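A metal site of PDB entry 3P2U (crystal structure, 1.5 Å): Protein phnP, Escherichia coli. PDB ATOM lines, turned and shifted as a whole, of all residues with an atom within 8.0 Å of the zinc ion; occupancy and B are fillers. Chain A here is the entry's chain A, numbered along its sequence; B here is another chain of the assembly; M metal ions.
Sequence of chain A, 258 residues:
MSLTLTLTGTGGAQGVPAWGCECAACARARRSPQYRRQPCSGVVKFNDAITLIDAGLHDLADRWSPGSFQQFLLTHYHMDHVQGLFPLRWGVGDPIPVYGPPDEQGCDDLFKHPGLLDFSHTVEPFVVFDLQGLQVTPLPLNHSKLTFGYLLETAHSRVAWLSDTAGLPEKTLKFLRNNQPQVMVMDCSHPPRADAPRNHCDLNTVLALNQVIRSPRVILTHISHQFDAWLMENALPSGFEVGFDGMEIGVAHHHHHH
The zinc ion is bound by a ring nitrogen (ND1) of His 225 (2.1 Å), the side-chain sulfur of Cys 26 (2.3 Å), the side-chain sulfur of Cys 21 (2.3 Å) and the side-chain sulfur of Cys 23 (2.4 Å).
The zinc ion has four donor atoms within binding distance.
The side-chain amide nitrogen (NE2) of Gln 226 sits close to a ring nitrogen (NE2) of His 225 (3.5 Å).
The side-chain amide oxygen (OE1) of Gln 14 sits close to a ring nitrogen (NE2) of His 225 (3.2 Å).
The side-chain sulfur (SG) of Cys 26 lies close to the backbone NH (N) of Ala 18, at 3.3 Å.
The backbone carbonyl oxygen of Cys 21 sits at hydrogen-bond distance from the guanidinium group of Arg 30, at 2.7 Å.
SG of Cys 23 sits close to N of Ala 25, 3.5 Å away.
Of the 21 residues printed, 4 come within 4 Å of the zinc ion.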
ATOM      1  N   GLN A  14       6.983 -21.179 -11.945  1.00  0.00           N
ATOM      2  CA  GLN A  14       6.430 -21.408 -13.274  1.00  0.00           C
ATOM      3  C   GLN A  14       7.449 -22.019 -14.231  1.00  0.00           C
ATOM      4  O   GLN A  14       7.100 -22.786 -15.126  1.00  0.00           O
ATOM      5  CB  GLN A  14       5.915 -20.082 -13.806  1.00  0.00           C
ATOM      6  CG  GLN A  14       5.372 -20.084 -15.235  1.00  0.00           C
ATOM      7  CD  GLN A  14       4.909 -18.696 -15.630  1.00  0.00           C
ATOM      8  OE1 GLN A  14       5.702 -17.743 -15.611  1.00  0.00           O
ATOM      9  NE2 GLN A  14       3.632 -18.550 -15.949  1.00  0.00           N
ATOM     10  N   GLY A  15       8.706 -21.630 -14.048  1.00  0.00           N
ATOM     11  CA  GLY A  15       9.787 -22.131 -14.881  1.00  0.00           C
ATOM     12  C   GLY A  15       9.851 -21.482 -16.252  1.00  0.00           C
ATOM     13  O   GLY A  15       8.965 -20.705 -16.639  1.00  0.00           O
ATOM     14  N   VAL A  16      10.916 -21.800 -16.978  1.00  0.00           N
ATOM     15  CA  VAL A  16      11.034 -21.495 -18.406  1.00  0.00           C
ATOM     16  C   VAL A  16      11.439 -22.804 -19.086  1.00  0.00           C
ATOM     17  O   VAL A  16      12.457 -23.376 -18.748  1.00  0.00           O
ATOM     18  CB  VAL A  16      12.117 -20.419 -18.690  1.00  0.00           C
ATOM     19  CG1 VAL A  16      12.155 -20.108 -20.177  1.00  0.00           C
ATOM     20  CG2 VAL A  16      11.851 -19.167 -17.869  1.00  0.00           C
ATOM     21  N   PRO A  17      10.644 -23.296 -20.032  1.00  0.00           N
ATOM     22  CA  PRO A  17       9.410 -22.671 -20.517  1.00  0.00           C
ATOM     23  C   PRO A  17       8.266 -22.823 -19.520  1.00  0.00           C
ATOM     24  O   PRO A  17       8.170 -23.812 -18.783  1.00  0.00           O
ATOM     25  CB  PRO A  17       9.087 -23.507 -21.769  1.00  0.00           C
ATOM     26  CG  PRO A  17       9.609 -24.896 -21.392  1.00  0.00           C
ATOM     27  CD  PRO A  17      10.901 -24.591 -20.675  1.00  0.00           C
ATOM     28  N   ALA A  18       7.387 -21.827 -19.511  1.00  0.00           N
ATOM     29  CA  ALA A  18       6.142 -21.932 -18.769  1.00  0.00           C
ATOM     30  C   ALA A  18       5.239 -22.889 -19.534  1.00  0.00           C
ATOM     31  O   ALA A  18       5.230 -22.879 -20.765  1.00  0.00           O
ATOM     32  CB  ALA A  18       5.492 -20.557 -18.646  1.00  0.00           C
ATOM     33  N   TRP A  19       4.511 -23.737 -18.829  1.00  0.00           N
ATOM     34  CA  TRP A  19       3.732 -24.790 -19.493  1.00  0.00           C
ATOM     35  C   TRP A  19       2.736 -24.181 -20.481  1.00  0.00           C
ATOM     36  O   TRP A  19       1.953 -23.302 -20.126  1.00  0.00           O
ATOM     37  CB  TRP A  19       3.001 -25.653 -18.467  1.00  0.00           C
ATOM     38  CG  TRP A  19       2.462 -26.942 -19.037  1.00  0.00           C
ATOM     39  CD1 TRP A  19       3.078 -27.783 -19.908  1.00  0.00           C
ATOM     40  CD2 TRP A  19       1.180 -27.514 -18.758  1.00  0.00           C
ATOM     41  NE1 TRP A  19       2.254 -28.865 -20.195  1.00  0.00           N
ATOM     42  CE2 TRP A  19       1.080 -28.721 -19.501  1.00  0.00           C
ATOM     43  CE3 TRP A  19       0.111 -27.147 -17.946  1.00  0.00           C
ATOM     44  CZ2 TRP A  19      -0.044 -29.534 -19.445  1.00  0.00           C
ATOM     45  CZ3 TRP A  19      -1.011 -27.962 -17.900  1.00  0.00           C
ATOM     46  CH2 TRP A  19      -1.081 -29.148 -18.649  1.00  0.00           C
ATOM     47  N   GLY A  20       2.799 -24.638 -21.718  1.00  0.00           N
ATOM     48  CA  GLY A  20       1.898 -24.164 -22.751  1.00  0.00           C
ATOM     49  C   GLY A  20       2.229 -22.821 -23.389  1.00  0.00           C
ATOM     50  O   GLY A  20       1.629 -22.460 -24.392  1.00  0.00           O
ATOM     51  N   CYS A  21       3.179 -22.083 -22.812  1.00  0.00           N
ATOM     52  CA  CYS A  21       3.508 -20.767 -23.355  1.00  0.00           C
ATOM     53  C   CYS A  21       4.383 -20.867 -24.595  1.00  0.00           C
ATOM     54  O   CYS A  21       5.313 -21.659 -24.640  1.00  0.00           O
ATOM     55  CB  CYS A  21       4.215 -19.904 -22.311  1.00  0.00           C
ATOM     56  SG  CYS A  21       4.481 -18.213 -22.885  1.00  0.00           S
ATOM     57  N   GLU A  22       4.096 -20.035 -25.591  1.00  0.00           N
ATOM     58  CA  GLU A  22       4.881 -20.003 -26.806  1.00  0.00           C
ATOM     59  C   GLU A  22       5.484 -18.627 -27.059  1.00  0.00           C
ATOM     60  O   GLU A  22       5.770 -18.254 -28.201  1.00  0.00           O
ATOM     61  CB  GLU A  22       4.042 -20.459 -27.993  1.00  0.00           C
ATOM     62  CG  GLU A  22       3.522 -21.870 -27.811  1.00  0.00           C
ATOM     63  CD  GLU A  22       3.670 -22.701 -29.053  1.00  0.00           C
ATOM     64  OE1 GLU A  22       4.795 -23.140 -29.349  1.00  0.00           O
ATOM     65  OE2 GLU A  22       2.649 -22.904 -29.745  1.00  0.00           O
ATOM     66  N   CYS A  23       5.706 -17.869 -25.984  1.00  0.00           N
ATOM     67  CA  CYS A  23       6.397 -16.596 -26.133  1.00  0.00           C
ATOM     68  C   CYS A  23       7.819 -16.846 -26.625  1.00  0.00           C
ATOM     69  O   CYS A  23       8.268 -17.992 -26.667  1.00  0.00           O
ATOM     70  CB  CYS A  23       6.392 -15.784 -24.836  1.00  0.00           C
ATOM     71  SG  CYS A  23       7.668 -16.264 -23.648  1.00  0.00           S
ATOM     72  N   ALA A  24       8.502 -15.786 -27.036  1.00  0.00           N
ATOM     73  CA  ALA A  24       9.837 -15.932 -27.592  1.00  0.00           C
ATOM     74  C   ALA A  24      10.793 -16.688 -26.655  1.00  0.00           C
ATOM     75  O   ALA A  24      11.573 -17.507 -27.122  1.00  0.00           O
ATOM     76  CB  ALA A  24      10.400 -14.567 -27.955  1.00  0.00           C
ATOM     77  N   ALA A  25      10.721 -16.418 -25.354  1.00  0.00           N
ATOM     78  CA  ALA A  25      11.636 -17.072 -24.409  1.00  0.00           C
ATOM     79  C   ALA A  25      11.279 -18.544 -24.224  1.00  0.00           C
ATOM     80  O   ALA A  25      12.157 -19.411 -24.219  1.00  0.00           O
ATOM     81  CB  ALA A  25      11.631 -16.355 -23.079  1.00  0.00           C
ATOM     82  N   CYS A  26       9.993 -18.832 -24.076  1.00  0.00           N
ATOM     83  CA  CYS A  26       9.569 -20.213 -23.845  1.00  0.00           C
ATOM     84  C   CYS A  26       9.763 -21.093 -25.081  1.00  0.00           C
ATOM     85  O   CYS A  26      10.217 -22.233 -24.969  1.00  0.00           O
ATOM     86  CB  CYS A  26       8.133 -20.267 -23.347  1.00  0.00           C
ATOM     87  SG  CYS A  26       7.966 -19.507 -21.718  1.00  0.00           S
ATOM     88  N   ALA A  27       9.422 -20.570 -26.256  1.00  0.00           N
ATOM     89  CA  ALA A  27       9.648 -21.323 -27.481  1.00  0.00           C
ATOM     90  C   ALA A  27      11.141 -21.628 -27.652  1.00  0.00           C
ATOM     91  O   ALA A  27      11.506 -22.746 -28.004  1.00  0.00           O
ATOM     92  CB  ALA A  27       9.096 -20.562 -28.691  1.00  0.00           C
ATOM     93  N   ARG A  30      12.201 -24.434 -25.343  1.00  0.00           N
ATOM     94  CA  ARG A  30      11.763 -25.757 -25.804  1.00  0.00           C
ATOM     95  C   ARG A  30      12.675 -26.281 -26.898  1.00  0.00           C
ATOM     96  O   ARG A  30      12.942 -27.487 -26.962  1.00  0.00           O
ATOM     97  CB  ARG A  30      10.322 -25.729 -26.329  1.00  0.00           C
ATOM     98  CG  ARG A  30       9.324 -25.760 -25.222  1.00  0.00           C
ATOM     99  CD  ARG A  30       7.929 -26.248 -25.639  1.00  0.00           C
ATOM    100  NE  ARG A  30       7.072 -25.819 -24.551  1.00  0.00           N
ATOM    101  CZ  ARG A  30       6.552 -24.602 -24.472  1.00  0.00           C
ATOM    102  NH1 ARG A  30       6.733 -23.754 -25.471  1.00  0.00           N
ATOM    103  NH2 ARG A  30       5.816 -24.264 -23.428  1.00  0.00           N
ATOM    104  N   SER A 224      11.622 -14.900 -14.530  1.00  0.00           N
ATOM    105  CA  SER A 224      10.370 -15.293 -15.187  1.00  0.00           C
ATOM    106  C   SER A 224      10.529 -15.263 -16.693  1.00  0.00           C
ATOM    107  O   SER A 224      11.424 -14.589 -17.235  1.00  0.00           O
ATOM    108  CB  SER A 224       9.238 -14.334 -14.816  1.00  0.00           C
ATOM    109  OG  SER A 224       9.382 -13.083 -15.493  1.00  0.00           O
ATOM    110  N   HIS A 225       9.636 -15.986 -17.383  1.00  0.00           N
ATOM    111  CA  HIS A 225       9.681 -15.964 -18.841  1.00  0.00           C
ATOM    112  C   HIS A 225       9.498 -14.553 -19.435  1.00  0.00           C
ATOM    113  O   HIS A 225      10.092 -14.260 -20.479  1.00  0.00           O
ATOM    114  CB  HIS A 225       8.718 -16.968 -19.489  1.00  0.00           C
ATOM    115  CG  HIS A 225       7.258 -16.694 -19.235  1.00  0.00           C
ATOM    116  ND1 HIS A 225       6.293 -16.909 -20.192  1.00  0.00           N
ATOM    117  CD2 HIS A 225       6.605 -16.267 -18.133  1.00  0.00           C
ATOM    118  CE1 HIS A 225       5.107 -16.629 -19.683  1.00  0.00           C
ATOM    119  NE2 HIS A 225       5.271 -16.237 -18.439  1.00  0.00           N
ATOM    120  N   GLN A 226       8.722 -13.705 -18.776  1.00  0.00           N
ATOM    121  CA  GLN A 226       8.559 -12.327 -19.238  1.00  0.00           C
ATOM    122  C   GLN A 226       9.874 -11.549 -19.196  1.00  0.00           C
ATOM    123  O   GLN A 226      10.191 -10.758 -20.086  1.00  0.00           O
ATOM    124  CB  GLN A 226       7.519 -11.584 -18.396  1.00  0.00           C
ATOM    125  CG  GLN A 226       6.089 -12.090 -18.581  1.00  0.00           C
ATOM    126  CD  GLN A 226       5.584 -12.937 -17.436  1.00  0.00           C
ATOM    127  OE1 GLN A 226       4.374 -13.081 -17.249  1.00  0.00           O
ATOM    128  NE2 GLN A 226       6.499 -13.515 -16.677  1.00  0.00           N
ATOM    129  N   ASP A 228      12.889 -12.991 -19.268  1.00  0.00           N
ATOM    130  CA  ASP A 228      13.745 -13.567 -20.306  1.00  0.00           C
ATOM    131  C   ASP A 228      13.429 -12.977 -21.690  1.00  0.00           C
ATOM    132  O   ASP A 228      14.344 -12.697 -22.476  1.00  0.00           O
ATOM    133  CB  ASP A 228      13.595 -15.075 -20.370  1.00  0.00           C
ATOM    134  CG  ASP A 228      14.706 -15.806 -19.692  1.00  0.00           C
ATOM    135  OD1 ASP A 228      15.794 -15.224 -19.519  1.00  0.00           O
ATOM    136  OD2 ASP A 228      14.463 -16.971 -19.347  1.00  0.00           O
ATOM    137  N   ALA A 229      12.147 -12.828 -21.990  1.00  0.00           N
ATOM    138  CA  ALA A 229      11.754 -12.215 -23.259  1.00  0.00           C
ATOM    139  C   ALA A 229      12.283 -10.782 -23.360  1.00  0.00           C
ATOM    140  O   ALA A 229      12.740 -10.363 -24.419  1.00  0.00           O
ATOM    141  CB  ALA A 229      10.240 -12.250 -23.431  1.00  0.00           C
ATOM    142  N   VAL B  92      -0.084 -21.611 -19.429  1.00  0.00           N
ATOM    143  CA  VAL B  92      -0.873 -20.799 -20.336  1.00  0.00           C
ATOM    144  C   VAL B  92      -1.851 -21.706 -21.083  1.00  0.00           C
ATOM    145  O   VAL B  92      -1.435 -22.685 -21.721  1.00  0.00           O
ATOM    146  CB  VAL B  92       0.037 -20.099 -21.353  1.00  0.00           C
ATOM    147  CG1 VAL B  92      -0.795 -19.419 -22.448  1.00  0.00           C
ATOM    148  CG2 VAL B  92       0.962 -19.099 -20.651  1.00  0.00           C
HETATM  149 ZN    ZN M   1       6.610 -17.718 -22.123  1.00  0.00          ZN
